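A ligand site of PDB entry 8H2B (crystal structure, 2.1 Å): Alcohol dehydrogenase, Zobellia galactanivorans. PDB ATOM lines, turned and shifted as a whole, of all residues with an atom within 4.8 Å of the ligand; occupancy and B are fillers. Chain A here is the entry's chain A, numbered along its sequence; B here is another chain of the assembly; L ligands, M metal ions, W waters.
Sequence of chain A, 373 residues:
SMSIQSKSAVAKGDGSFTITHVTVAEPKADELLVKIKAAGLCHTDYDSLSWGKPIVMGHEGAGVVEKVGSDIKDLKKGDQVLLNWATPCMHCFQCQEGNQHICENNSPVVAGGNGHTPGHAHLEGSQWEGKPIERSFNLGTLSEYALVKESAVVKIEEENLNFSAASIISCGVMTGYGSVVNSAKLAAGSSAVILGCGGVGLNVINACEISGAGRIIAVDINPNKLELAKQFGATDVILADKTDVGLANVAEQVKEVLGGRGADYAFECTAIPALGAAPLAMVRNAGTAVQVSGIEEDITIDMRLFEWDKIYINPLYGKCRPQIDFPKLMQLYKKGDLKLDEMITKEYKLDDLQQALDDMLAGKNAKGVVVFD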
ATOM      1  N   CYS A  42      23.433 -37.605   4.769  1.00  0.00           N
ATOM      2  CA  CYS A  42      24.004 -36.289   4.591  1.00  0.00           C
ATOM      3  C   CYS A  42      25.455 -36.352   5.029  1.00  0.00           C
ATOM      4  O   CYS A  42      25.821 -37.211   5.837  1.00  0.00           O
ATOM      5  CB  CYS A  42      23.208 -35.269   5.413  1.00  0.00           C
ATOM      6  SG  CYS A  42      23.774 -33.593   5.337  1.00  0.00           S
ATOM      7  N   HIS A  43      26.306 -35.461   4.500  1.00  0.00           N
ATOM      8  CA  HIS A  43      27.690 -35.438   4.951  1.00  0.00           C
ATOM      9  C   HIS A  43      27.781 -35.222   6.458  1.00  0.00           C
ATOM     10  O   HIS A  43      28.705 -35.732   7.108  1.00  0.00           O
ATOM     11  CB  HIS A  43      28.489 -34.349   4.213  1.00  0.00           C
ATOM     12  CG  HIS A  43      29.981 -34.431   4.444  1.00  0.00           C
ATOM     13  ND1 HIS A  43      30.580 -34.054   5.623  1.00  0.00           N
ATOM     14  CD2 HIS A  43      30.979 -34.851   3.634  1.00  0.00           C
ATOM     15  CE1 HIS A  43      31.877 -34.236   5.541  1.00  0.00           C
ATOM     16  NE2 HIS A  43      32.158 -34.724   4.339  1.00  0.00           N
ATOM     17  N   THR A  44      26.808 -34.498   7.043  1.00  0.00           N
ATOM     18  CA  THR A  44      26.844 -34.190   8.463  1.00  0.00           C
ATOM     19  C   THR A  44      26.649 -35.439   9.338  1.00  0.00           C
ATOM     20  O   THR A  44      27.115 -35.471  10.476  1.00  0.00           O
ATOM     21  CB  THR A  44      25.787 -33.133   8.784  1.00  0.00           C
ATOM     22  OG1 THR A  44      25.865 -32.079   7.804  1.00  0.00           O
ATOM     23  CG2 THR A  44      25.981 -32.545  10.159  1.00  0.00           C
ATOM     24  N   ASP A  47      30.060 -36.406  10.019  1.00  0.00           N
ATOM     25  CA  ASP A  47      30.622 -35.575  11.085  1.00  0.00           C
ATOM     26  C   ASP A  47      30.021 -35.923  12.443  1.00  0.00           C
ATOM     27  O   ASP A  47      30.667 -35.687  13.468  1.00  0.00           O
ATOM     28  CB  ASP A  47      30.413 -34.077  10.806  1.00  0.00           C
ATOM     29  CG  ASP A  47      30.733 -33.666   9.367  1.00  0.00           C
ATOM     30  OD1 ASP A  47      31.893 -33.875   8.924  1.00  0.00           O
ATOM     31  OD2 ASP A  47      29.831 -33.144   8.678  1.00  0.00           O
ATOM     32  N   TRP A  85      14.262 -30.822  10.671  1.00  0.00           N
ATOM     33  CA  TRP A  85      15.016 -30.665  11.916  1.00  0.00           C
ATOM     34  C   TRP A  85      15.013 -29.235  12.436  1.00  0.00           C
ATOM     35  O   TRP A  85      15.736 -28.938  13.375  1.00  0.00           O
ATOM     36  CB  TRP A  85      16.453 -31.171  11.781  1.00  0.00           C
ATOM     37  CG  TRP A  85      17.279 -30.751  10.609  1.00  0.00           C
ATOM     38  CD1 TRP A  85      17.458 -31.447   9.433  1.00  0.00           C
ATOM     39  CD2 TRP A  85      18.134 -29.593  10.515  1.00  0.00           C
ATOM     40  NE1 TRP A  85      18.334 -30.773   8.610  1.00  0.00           N
ATOM     41  CE2 TRP A  85      18.772 -29.640   9.259  1.00  0.00           C
ATOM     42  CE3 TRP A  85      18.413 -28.522  11.375  1.00  0.00           C
ATOM     43  CZ2 TRP A  85      19.663 -28.647   8.831  1.00  0.00           C
ATOM     44  CZ3 TRP A  85      19.299 -27.537  10.946  1.00  0.00           C
ATOM     45  CH2 TRP A  85      19.922 -27.610   9.700  1.00  0.00           C
ATOM     46  N   CYS A 171      16.917 -32.586   4.234  1.00  0.00           N
ATOM     47  CA  CYS A 171      18.103 -31.768   4.453  1.00  0.00           C
ATOM     48  C   CYS A 171      18.762 -31.293   3.157  1.00  0.00           C
ATOM     49  O   CYS A 171      18.811 -30.086   2.893  1.00  0.00           O
ATOM     50  CB  CYS A 171      19.137 -32.499   5.286  1.00  0.00           C
ATOM     51  SG  CYS A 171      20.464 -31.399   5.810  1.00  0.00           S
ATOM     52  N   THR A 175      18.168 -27.564   1.959  1.00  0.00           N
ATOM     53  CA  THR A 175      19.306 -26.672   2.163  1.00  0.00           C
ATOM     54  C   THR A 175      19.802 -26.123   0.833  1.00  0.00           C
ATOM     55  O   THR A 175      20.069 -24.920   0.716  1.00  0.00           O
ATOM     56  CB  THR A 175      20.439 -27.411   2.873  1.00  0.00           C
ATOM     57  OG1 THR A 175      20.035 -27.805   4.196  1.00  0.00           O
ATOM     58  CG2 THR A 175      21.685 -26.533   2.935  1.00  0.00           C
ATOM     59  N   LEU A 195      30.286 -24.475  -6.181  1.00  0.00           N
ATOM     60  CA  LEU A 195      31.559 -25.060  -5.775  1.00  0.00           C
ATOM     61  C   LEU A 195      31.257 -26.270  -4.888  1.00  0.00           C
ATOM     62  O   LEU A 195      30.841 -26.096  -3.728  1.00  0.00           O
ATOM     63  CB  LEU A 195      32.403 -24.052  -5.013  1.00  0.00           C
ATOM     64  CG  LEU A 195      32.600 -22.692  -5.680  1.00  0.00           C
ATOM     65  CD1 LEU A 195      33.352 -21.773  -4.733  1.00  0.00           C
ATOM     66  CD2 LEU A 195      33.364 -22.870  -6.985  1.00  0.00           C
ATOM     67  N   GLY A 196      31.503 -27.471  -5.425  1.00  0.00           N
ATOM     68  CA  GLY A 196      31.192 -28.707  -4.739  1.00  0.00           C
ATOM     69  C   GLY A 196      29.859 -29.271  -5.165  1.00  0.00           C
ATOM     70  O   GLY A 196      28.807 -28.729  -4.792  1.00  0.00           O
ATOM     71  N   CYS A 197      29.869 -30.352  -5.943  1.00  0.00           N
ATOM     72  CA  CYS A 197      28.647 -30.908  -6.521  1.00  0.00           C
ATOM     73  C   CYS A 197      28.250 -32.210  -5.829  1.00  0.00           C
ATOM     74  O   CYS A 197      28.147 -33.249  -6.486  1.00  0.00           O
ATOM     75  CB  CYS A 197      28.820 -31.129  -8.018  1.00  0.00           C
ATOM     76  SG  CYS A 197      29.216 -29.603  -8.915  1.00  0.00           S
ATOM     77  N   GLY A 198      28.017 -32.158  -4.524  1.00  0.00           N
ATOM     78  CA  GLY A 198      27.619 -33.287  -3.716  1.00  0.00           C
ATOM     79  C   GLY A 198      26.148 -33.264  -3.372  1.00  0.00           C
ATOM     80  O   GLY A 198      25.318 -32.770  -4.156  1.00  0.00           O
ATOM     81  N   GLY A 199      25.822 -33.759  -2.172  1.00  0.00           N
ATOM     82  CA  GLY A 199      24.421 -33.847  -1.790  1.00  0.00           C
ATOM     83  C   GLY A 199      23.727 -32.499  -1.790  1.00  0.00           C
ATOM     84  O   GLY A 199      22.600 -32.347  -2.267  1.00  0.00           O
ATOM     85  N   VAL A 200      24.401 -31.479  -1.262  1.00  0.00           N
ATOM     86  CA  VAL A 200      23.813 -30.146  -1.254  1.00  0.00           C
ATOM     87  C   VAL A 200      24.000 -29.474  -2.609  1.00  0.00           C
ATOM     88  O   VAL A 200      23.046 -28.923  -3.182  1.00  0.00           O
ATOM     89  CB  VAL A 200      24.419 -29.309  -0.115  1.00  0.00           C
ATOM     90  CG1 VAL A 200      23.997 -27.873  -0.247  1.00  0.00           C
ATOM     91  CG2 VAL A 200      23.991 -29.875   1.250  1.00  0.00           C
ATOM     92  N   GLY A 201      25.219 -29.518  -3.151  1.00  0.00           N
ATOM     93  CA  GLY A 201      25.522 -28.789  -4.368  1.00  0.00           C
ATOM     94  C   GLY A 201      24.671 -29.180  -5.565  1.00  0.00           C
ATOM     95  O   GLY A 201      24.277 -28.327  -6.364  1.00  0.00           O
ATOM     96  N   VAL A 219      31.518 -26.865 -10.392  1.00  0.00           N
ATOM     97  CA  VAL A 219      32.930 -26.994 -10.095  1.00  0.00           C
ATOM     98  C   VAL A 219      33.097 -28.123  -9.086  1.00  0.00           C
ATOM     99  O   VAL A 219      32.449 -28.101  -8.030  1.00  0.00           O
ATOM    100  CB  VAL A 219      33.503 -25.684  -9.520  1.00  0.00           C
ATOM    101  CG1 VAL A 219      34.956 -25.851  -9.140  1.00  0.00           C
ATOM    102  CG2 VAL A 219      33.250 -24.494 -10.458  1.00  0.00           C
ATOM    103  N   ASP A 220      33.948 -29.094  -9.403  1.00  0.00           N
ATOM    104  CA  ASP A 220      34.258 -30.144  -8.435  1.00  0.00           C
ATOM    105  C   ASP A 220      35.642 -30.721  -8.713  1.00  0.00           C
ATOM    106  O   ASP A 220      36.187 -30.589  -9.819  1.00  0.00           O
ATOM    107  CB  ASP A 220      33.203 -31.263  -8.458  1.00  0.00           C
ATOM    108  CG  ASP A 220      33.040 -31.973  -7.100  1.00  0.00           C
ATOM    109  OD1 ASP A 220      33.993 -32.706  -6.684  1.00  0.00           O
ATOM    110  OD2 ASP A 220      31.950 -31.856  -6.480  1.00  0.00           O
ATOM    111  N   ILE A 221      36.214 -31.380  -7.704  1.00  0.00           N
ATOM    112  CA  ILE A 221      37.467 -32.090  -7.928  1.00  0.00           C
ATOM    113  C   ILE A 221      37.251 -33.471  -8.526  1.00  0.00           C
ATOM    114  O   ILE A 221      38.220 -34.102  -8.963  1.00  0.00           O
ATOM    115  CB  ILE A 221      38.285 -32.193  -6.633  1.00  0.00           C
ATOM    116  CG1 ILE A 221      37.419 -32.786  -5.500  1.00  0.00           C
ATOM    117  CG2 ILE A 221      38.849 -30.827  -6.240  1.00  0.00           C
ATOM    118  CD1 ILE A 221      38.227 -33.171  -4.269  1.00  0.00           C
ATOM    119  N   ASN A 222      36.006 -33.932  -8.596  1.00  0.00           N
ATOM    120  CA  ASN A 222      35.663 -35.300  -8.992  1.00  0.00           C
ATOM    121  C   ASN A 222      34.917 -35.297 -10.321  1.00  0.00           C
ATOM    122  O   ASN A 222      33.817 -34.729 -10.413  1.00  0.00           O
ATOM    123  CB  ASN A 222      34.813 -35.948  -7.887  1.00  0.00           C
ATOM    124  CG  ASN A 222      34.532 -37.426  -8.136  1.00  0.00           C
ATOM    125  OD1 ASN A 222      34.448 -37.874  -9.285  1.00  0.00           O
ATOM    126  ND2 ASN A 222      34.379 -38.182  -7.067  1.00  0.00           N
ATOM    127  N   LYS A 225      31.228 -36.317 -10.306  1.00  0.00           N
ATOM    128  CA  LYS A 225      30.276 -35.350  -9.795  1.00  0.00           C
ATOM    129  C   LYS A 225      29.914 -34.325 -10.867  1.00  0.00           C
ATOM    130  O   LYS A 225      28.773 -33.861 -10.930  1.00  0.00           O
ATOM    131  CB  LYS A 225      30.842 -34.665  -8.555  1.00  0.00           C
ATOM    132  CG  LYS A 225      31.009 -35.612  -7.379  1.00  0.00           C
ATOM    133  CD  LYS A 225      29.646 -36.119  -6.926  1.00  0.00           C
ATOM    134  CE  LYS A 225      29.757 -36.976  -5.706  1.00  0.00           C
ATOM    135  NZ  LYS A 225      30.282 -36.195  -4.551  1.00  0.00           N
ATOM    136  N   ALA A 240      38.198 -28.850 -10.834  1.00  0.00           N
ATOM    137  CA  ALA A 240      39.165 -28.137 -10.007  1.00  0.00           C
ATOM    138  C   ALA A 240      40.306 -29.048  -9.623  1.00  0.00           C
ATOM    139  O   ALA A 240      40.186 -30.278  -9.635  1.00  0.00           O
ATOM    140  CB  ALA A 240      38.509 -27.568  -8.753  1.00  0.00           C
ATOM    141  N   LYS A 242      42.564 -30.062  -6.408  1.00  0.00           N
ATOM    142  CA  LYS A 242      42.683 -30.024  -4.955  1.00  0.00           C
ATOM    143  C   LYS A 242      43.735 -29.040  -4.469  1.00  0.00           C
ATOM    144  O   LYS A 242      43.563 -28.427  -3.412  1.00  0.00           O
ATOM    145  CB  LYS A 242      42.958 -31.438  -4.463  1.00  0.00           C
ATOM    146  CG  LYS A 242      41.776 -32.330  -4.560  1.00  0.00           C
ATOM    147  CD  LYS A 242      42.224 -33.702  -4.287  1.00  0.00           C
ATOM    148  CE  LYS A 242      42.684 -33.772  -2.798  1.00  0.00           C
ATOM    149  NZ  LYS A 242      41.644 -33.481  -1.847  1.00  0.00           N
ATOM    150  N   LEU A 247      40.528 -21.879  -4.669  1.00  0.00           N
ATOM    151  CA  LEU A 247      39.970 -22.032  -6.010  1.00  0.00           C
ATOM    152  C   LEU A 247      40.213 -20.800  -6.882  1.00  0.00           C
ATOM    153  O   LEU A 247      39.407 -20.458  -7.750  1.00  0.00           O
ATOM    154  CB  LEU A 247      38.472 -22.371  -5.951  1.00  0.00           C
ATOM    155  CG  LEU A 247      38.138 -23.731  -5.304  1.00  0.00           C
ATOM    156  CD1 LEU A 247      36.646 -23.879  -5.089  1.00  0.00           C
ATOM    157  CD2 LEU A 247      38.650 -24.897  -6.144  1.00  0.00           C
ATOM    158  N   CYS A 269      29.866 -25.364  -1.298  1.00  0.00           N
ATOM    159  CA  CYS A 269      29.209 -26.588  -0.848  1.00  0.00           C
ATOM    160  C   CYS A 269      30.219 -27.710  -0.659  1.00  0.00           C
ATOM    161  O   CYS A 269      29.855 -28.884  -0.831  1.00  0.00           O
ATOM    162  CB  CYS A 269      28.210 -27.092  -1.903  1.00  0.00           C
ATOM    163  SG  CYS A 269      26.957 -25.960  -2.450  1.00  0.00           S
ATOM    164  N   THR A 270      31.473 -27.398  -0.364  1.00  0.00           N
ATOM    165  CA  THR A 270      32.545 -28.385  -0.515  1.00  0.00           C
ATOM    166  C   THR A 270      32.883 -29.145   0.760  1.00  0.00           C
ATOM    167  O   THR A 270      33.603 -30.147   0.673  1.00  0.00           O
ATOM    168  CB  THR A 270      33.835 -27.730  -0.997  1.00  0.00           C
ATOM    169  OG1 THR A 270      34.356 -26.910   0.066  1.00  0.00           O
ATOM    170  CG2 THR A 270      33.578 -26.868  -2.258  1.00  0.00           C
ATOM    171  N   ALA A 271      32.423 -28.690   1.929  1.00  0.00           N
ATOM    172  CA  ALA A 271      32.824 -29.220   3.234  1.00  0.00           C
ATOM    173  C   ALA A 271      34.306 -28.974   3.537  1.00  0.00           C
ATOM    174  O   ALA A 271      34.853 -29.570   4.463  1.00  0.00           O
ATOM    175  CB  ALA A 271      32.502 -30.716   3.353  1.00  0.00           C
ATOM    176  N   ILE A 272      34.966 -28.081   2.804  1.00  0.00           N
ATOM    177  CA  ILE A 272      36.388 -27.796   2.991  1.00  0.00           C
ATOM    178  C   ILE A 272      36.517 -26.448   3.703  1.00  0.00           C
ATOM    179  O   ILE A 272      36.298 -25.413   3.063  1.00  0.00           O
ATOM    180  CB  ILE A 272      37.137 -27.768   1.641  1.00  0.00           C
ATOM    181  CG1 ILE A 272      37.009 -29.117   0.909  1.00  0.00           C
ATOM    182  CG2 ILE A 272      38.610 -27.375   1.840  1.00  0.00           C
ATOM    183  CD1 ILE A 272      37.465 -30.354   1.742  1.00  0.00           C
ATOM    184  N   LEU A 275      38.064 -23.401   2.035  1.00  0.00           N
ATOM    185  CA  LEU A 275      37.421 -22.847   0.852  1.00  0.00           C
ATOM    186  C   LEU A 275      36.254 -21.912   1.208  1.00  0.00           C
ATOM    187  O   LEU A 275      35.407 -21.616   0.358  1.00  0.00           O
ATOM    188  CB  LEU A 275      36.955 -23.969  -0.080  1.00  0.00           C
ATOM    189  CG  LEU A 275      38.053 -24.775  -0.774  1.00  0.00           C
ATOM    190  CD1 LEU A 275      37.444 -25.766  -1.720  1.00  0.00           C
ATOM    191  CD2 LEU A 275      38.986 -23.880  -1.558  1.00  0.00           C
ATOM    192  N   VAL A 292      27.553 -22.402   2.069  1.00  0.00           N
ATOM    193  CA  VAL A 292      26.547 -23.295   2.627  1.00  0.00           C
ATOM    194  C   VAL A 292      27.123 -24.283   3.633  1.00  0.00           C
ATOM    195  O   VAL A 292      26.377 -24.813   4.473  1.00  0.00           O
ATOM    196  CB  VAL A 292      25.807 -24.043   1.486  1.00  0.00           C
ATOM    197  CG1 VAL A 292      24.683 -24.901   2.035  1.00  0.00           C
ATOM    198  CG2 VAL A 292      25.240 -23.038   0.490  1.00  0.00           C
ATOM    199  N   SER A 293      28.444 -24.514   3.614  1.00  0.00           N
ATOM    200  CA  SER A 293      29.012 -25.608   4.392  1.00  0.00           C
ATOM    201  C   SER A 293      28.870 -25.394   5.891  1.00  0.00           C
ATOM    202  O   SER A 293      28.583 -26.343   6.643  1.00  0.00           O
ATOM    203  CB  SER A 293      30.486 -25.807   4.032  1.00  0.00           C
ATOM    204  OG  SER A 293      30.623 -26.429   2.772  1.00  0.00           O
ATOM    205  N   PRO A 315      23.994 -19.180   5.329  1.00  0.00           N
ATOM    206  CA  PRO A 315      22.657 -19.518   5.831  1.00  0.00           C
ATOM    207  C   PRO A 315      22.564 -20.937   6.377  1.00  0.00           C
ATOM    208  O   PRO A 315      23.314 -21.834   5.980  1.00  0.00           O
ATOM    209  CB  PRO A 315      21.772 -19.342   4.599  1.00  0.00           C
ATOM    210  CG  PRO A 315      22.721 -19.679   3.422  1.00  0.00           C
ATOM    211  CD  PRO A 315      24.112 -19.370   3.868  1.00  0.00           C
ATOM    212  N   LEU A 316      21.641 -21.121   7.316  1.00  0.00           N
ATOM    213  CA  LEU A 316      21.338 -22.418   7.894  1.00  0.00           C
ATOM    214  C   LEU A 316      20.083 -23.000   7.254  1.00  0.00           C
ATOM    215  O   LEU A 316      19.069 -22.308   7.135  1.00  0.00           O
ATOM    216  CB  LEU A 316      21.129 -22.315   9.411  1.00  0.00           C
ATOM    217  CG  LEU A 316      20.920 -23.646  10.147  1.00  0.00           C
ATOM    218  CD1 LEU A 316      22.116 -24.567   9.954  1.00  0.00           C
ATOM    219  CD2 LEU A 316      20.670 -23.415  11.658  1.00  0.00           C
ATOM    220  N   TYR A 317      20.181 -24.256   6.827  1.00  0.00           N
ATOM    221  CA  TYR A 317      19.028 -25.066   6.410  1.00  0.00           C
ATOM    222  C   TYR A 317      18.195 -24.366   5.331  1.00  0.00           C
ATOM    223  O   TYR A 317      16.975 -24.575   5.216  1.00  0.00           O
ATOM    224  CB  TYR A 317      18.215 -25.436   7.642  1.00  0.00           C
ATOM    225  CG  TYR A 317      17.198 -26.542   7.542  1.00  0.00           C
ATOM    226  CD1 TYR A 317      17.387 -27.610   6.677  1.00  0.00           C
ATOM    227  CD2 TYR A 317      16.304 -26.758   8.605  1.00  0.00           C
ATOM    228  CE1 TYR A 317      16.534 -28.698   6.678  1.00  0.00           C
ATOM    229  CE2 TYR A 317      15.466 -27.855   8.638  1.00  0.00           C
ATOM    230  CZ  TYR A 317      15.592 -28.826   7.686  1.00  0.00           C
ATOM    231  OH  TYR A 317      14.780 -29.939   7.721  1.00  0.00           O
ATOM    232  N   MET A 360      29.165 -42.434  -0.535  1.00  0.00           N
ATOM    233  CA  MET A 360      29.032 -40.989  -0.446  1.00  0.00           C
ATOM    234  C   MET A 360      30.400 -40.309  -0.441  1.00  0.00           C
ATOM    235  O   MET A 360      30.701 -39.470  -1.300  1.00  0.00           O
ATOM    236  CB  MET A 360      28.241 -40.608   0.812  1.00  0.00           C
ATOM    237  CG  MET A 360      28.288 -39.134   1.174  1.00  0.00           C
ATOM    238  SD  MET A 360      27.296 -38.709   2.637  1.00  0.00           S
ATOM    239  CE  MET A 360      28.428 -39.102   3.972  1.00  0.00           C
ATOM    240  N   TRP B 308      24.774 -17.370  12.216  1.00  0.00           N
ATOM    241  CA  TRP B 308      24.092 -17.837  10.984  1.00  0.00           C
ATOM    242  C   TRP B 308      23.241 -16.720  10.406  1.00  0.00           C
ATOM    243  O   TRP B 308      22.668 -15.875  11.098  1.00  0.00           O
ATOM    244  CB  TRP B 308      23.157 -19.045  11.263  1.00  0.00           C
ATOM    245  CG  TRP B 308      23.848 -20.263  11.791  1.00  0.00           C
ATOM    246  CD1 TRP B 308      23.920 -20.659  13.109  1.00  0.00           C
ATOM    247  CD2 TRP B 308      24.527 -21.274  11.030  1.00  0.00           C
ATOM    248  NE1 TRP B 308      24.636 -21.837  13.217  1.00  0.00           N
ATOM    249  CE2 TRP B 308      25.009 -22.238  11.949  1.00  0.00           C
ATOM    250  CE3 TRP B 308      24.770 -21.457   9.658  1.00  0.00           C
ATOM    251  CZ2 TRP B 308      25.725 -23.371  11.544  1.00  0.00           C
ATOM    252  CZ3 TRP B 308      25.491 -22.582   9.254  1.00  0.00           C
ATOM    253  CH2 TRP B 308      25.964 -23.518  10.191  1.00  0.00           C
HETATM  254  P1  LIG L   1      29.240 -34.087  -0.020  1.00  0.00           P
HETATM  255  O1  LIG L   1      30.402 -34.863   0.503  1.00  0.00           O
HETATM  256  O2  LIG L   1      28.135 -34.921  -0.614  1.00  0.00           O
HETATM  257  O3  LIG L   1      29.699 -33.009  -1.203  1.00  0.00           O
HETATM  258  C1  LIG L   1      30.928 -32.343  -1.048  1.00  0.00           C
HETATM  259  C2  LIG L   1      31.356 -32.053  -2.538  1.00  0.00           C
HETATM  260  O4  LIG L   1      32.295 -31.132  -2.529  1.00  0.00           O
HETATM  261  C3  LIG L   1      31.940 -33.324  -3.159  1.00  0.00           C
HETATM  262  O5  LIG L   1      31.448 -33.588  -4.413  1.00  0.00           O
HETATM  263  C4  LIG L   1      33.445 -32.978  -3.258  1.00  0.00           C
HETATM  264  O6  LIG L   1      33.994 -33.788  -4.373  1.00  0.00           O
HETATM  265  C5  LIG L   1      33.426 -31.707  -3.518  1.00  0.00           C
HETATM  266  N1  LIG L   1      34.709 -31.017  -3.279  1.00  0.00           N
HETATM  267  C6  LIG L   1      35.548 -31.369  -2.307  1.00  0.00           C
HETATM  268  N2  LIG L   1      36.638 -30.558  -2.376  1.00  0.00           N
HETATM  269  C7  LIG L   1      36.453 -29.720  -3.410  1.00  0.00           C
HETATM  270  C8  LIG L   1      37.240 -28.698  -3.927  1.00  0.00           C
HETATM  271  N3  LIG L   1      38.555 -28.275  -3.439  1.00  0.00           N
HETATM  272  N4  LIG L   1      36.813 -27.995  -4.966  1.00  0.00           N
HETATM  273  C9  LIG L   1      35.600 -28.279  -5.530  1.00  0.00           C
HETATM  274  N5  LIG L   1      34.824 -29.284  -5.033  1.00  0.00           N
HETATM  275  C10 LIG L   1      35.258 -29.991  -3.963  1.00  0.00           C
HETATM  276  O7  LIG L   1      28.649 -33.267   1.243  1.00  0.00           O
HETATM  277  P2  LIG L   1      27.207 -32.511   1.272  1.00  0.00           P
HETATM  278  O8  LIG L   1      26.172 -33.479   1.779  1.00  0.00           O
HETATM  279  O9  LIG L   1      26.823 -32.000  -0.101  1.00  0.00           O
HETATM  280  O10 LIG L   1      27.434 -31.285   2.315  1.00  0.00           O
HETATM  281  C11 LIG L   1      28.367 -30.297   2.040  1.00  0.00           C
HETATM  282  C12 LIG L   1      28.471 -29.397   3.221  1.00  0.00           C
HETATM  283  O11 LIG L   1      27.339 -28.771   3.486  1.00  0.00           O
HETATM  284  C13 LIG L   1      28.845 -30.283   4.562  1.00  0.00           C
HETATM  285  O12 LIG L   1      29.953 -29.556   5.208  1.00  0.00           O
HETATM  286  C14 LIG L   1      27.806 -30.325   5.269  1.00  0.00           C
HETATM  287  O13 LIG L   1      28.138 -30.377   6.729  1.00  0.00           O
HETATM  288  C15 LIG L   1      27.084 -28.930   4.955  1.00  0.00           C
HETATM  289  N6  LIG L   1      25.753 -28.847   5.157  1.00  0.00           N
HETATM  290  C16 LIG L   1      25.267 -27.653   5.607  1.00  0.00           C
HETATM  291  C17 LIG L   1      23.891 -27.474   5.774  1.00  0.00           C
HETATM  292  C18 LIG L   1      23.381 -26.093   6.288  1.00  0.00           C
HETATM  293  O14 LIG L   1      22.316 -26.023   6.831  1.00  0.00           O
HETATM  294  N7  LIG L   1      24.190 -24.871   6.090  1.00  0.00           N
HETATM  295  C19 LIG L   1      23.041 -28.500   5.494  1.00  0.00           C
HETATM  296  C20 LIG L   1      23.520 -29.689   5.033  1.00  0.00           C
HETATM  297  C21 LIG L   1      24.901 -29.859   4.867  1.00  0.00           C
HETATM  298 ZN    ZN M   1      22.245 -32.526   6.747  1.00  0.00          ZN
HETATM  299  O   HOH W   1      31.289 -30.573   7.344  1.00  0.00           O
HETATM  300  O   HOH W   2      23.224 -30.776   8.184  1.00  0.00           O
HETATM  301  O   HOH W   3      39.417 -31.502  -1.090  1.00  0.00           O
HETATM  302  O   HOH W   4      40.770 -26.751  -4.374  1.00  0.00           O
HETATM  303  O   HOH W   5      29.516 -28.174   8.004  1.00  0.00           O
HETATM  304  O   HOH W   6      27.806 -30.567  -1.976  1.00  0.00           O
HETATM  305  O   HOH W   7      41.042 -29.481  -1.908  1.00  0.00           O
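N of Tyr 317 lies within hydrogen-bond range of O14 of the ligand (2.8 Å).
An oxygen (O8) of the ligand sits at hydrogen-bond distance from the backbone NH of His 43 (3.4 Å).
The side-chain carboxylate (OD1) of Asp 220 lies within hydrogen-bond range of an oxygen (O6) of the ligand, at 2.6 Å.
An oxygen (O9) of the ligand sits at hydrogen-bond distance from the backbone NH (N) of Val 200 (2.7 Å).
N of Gly 199 is in hydrogen-bond range of O9 of the ligand.
N7 of the ligand sits at hydrogen-bond distance from O of Val 292 (2.7 Å).
The side-chain hydroxyl (OG1) of Thr 44 sits at hydrogen-bond distance from an oxygen (O13) of the ligand (3.0 Å).
An oxygen (O5) of the ligand is in hydrogen-bond range of the side-chain amino group (NZ) of Lys 225, 2.9 Å away.
A nitrogen (N7) of the ligand sits at hydrogen-bond distance from the backbone carbonyl oxygen (O) of Pro 315 (3.2 Å).
SG of Cys 171 sits close to NE1 of Trp 85 (3.6 Å).
The backbone NH (N) of Cys 269 lies within hydrogen-bond range of the backbone carbonyl oxygen (O) of Leu 195, at 2.7 Å.
The backbone carbonyl oxygen (O) of Asp 220 lies within hydrogen-bond range of the backbone NH (N) of Ala 240 (2.8 Å).
The side-chain carboxylate of Asp 220 sits at hydrogen-bond distance from the backbone NH of Cys 197, at 2.6 Å.
OD1 of Asp 220 is in hydrogen-bond range of N of Asn 222.
N of Ile 272 lies within hydrogen-bond range of OG1 of Thr 270 (3.0 Å).
O of Val 219 sits at hydrogen-bond distance from SG of Cys 197, at 3.7 Å.
The side-chain hydroxyl of Thr 175 is in hydrogen-bond range of the backbone carbonyl oxygen of Cys 171 (2.9 Å).
SG of Cys 42 touches C20 of the ligand (3.9 Å).
OD2 of Asp 47 touches O13 of the ligand (3.8 Å).
Cys 171 touches the ligand.
Thr 175 touches the ligand (OG1 to C19, 3.3 Å).
CA of Gly 196 touches O4 of the ligand (3.5 Å).
Cys 197 touches the ligand (C to O5, 3.8 Å).
Gly 198 touches the ligand.
CG2 of Ile 221 touches C8 of the ligand, 3.5 Å away.
CD2 of Leu 247 touches N4 of the ligand, at 3.8 Å.
Cys 269 touches the ligand (O to C11, 3.5 Å).
Thr 270 touches the ligand (CA to O4, 3.4 Å).
CB of Ala 271 touches O12 of the ligand, 3.4 Å away.
CG1 of Ile 272 touches N2 of the ligand (3.6 Å).
CD1 of Leu 275 touches N3 of the ligand (3.2 Å).
Ser 293 touches the ligand.
Leu 316 touches the ligand (CD1 to O14, 3.5 Å).
Hydrophobic or aromatic side chains that line the ligand: His 43, Val 200, Ile 221, Leu 247, Ala 271, Ile 272, Leu 275 and Leu 316.
Within 4 Å of the ligand: Cys 42, His 43, Thr 44, Asp 47, Cys 171, Thr 175, Gly 196, Cys 197, Gly 198, Gly 199, Val 200, Asp 220, Ile 221, Lys 225, Leu 247, Cys 269, Thr 270, Ala 271, Ile 272, Leu 275, Val 292, Ser 293, Pro 315, Leu 316 and Tyr 317.
Water W6 lies within hydrogen-bond range of an oxygen (O9) of the ligand (2.6 Å), the backbone carbonyl oxygen (O) of Cys 269 (2.9 Å), the backbone NH (N) of Gly 198 (3.0 Å) and the backbone NH (N) of Gly 201 (3.0 Å).
Water W1 lies within hydrogen-bond range of an oxygen (O12) of the ligand (2.7 Å) and the side-chain carboxylate of Asp 47 (3.2 Å).
Water W4 lies within hydrogen-bond range of N3 of the ligand (2.8 Å) and O of Lys 242 (3.4 Å).
Water W5 bridges the backbone carbonyl oxygen (O) of Ser 293 (2.5 Å) and an oxygen (O13) of the ligand (2.9 Å).
Water W7 bridges the backbone carbonyl oxygen of Lys 242 (3.1 Å) and a nitrogen (N3) of the ligand (3.2 Å).
Water W3 bridges the side-chain amino group (NZ) of Lys 242 (3.1 Å) and a nitrogen (N2) of the ligand (3.2 Å).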
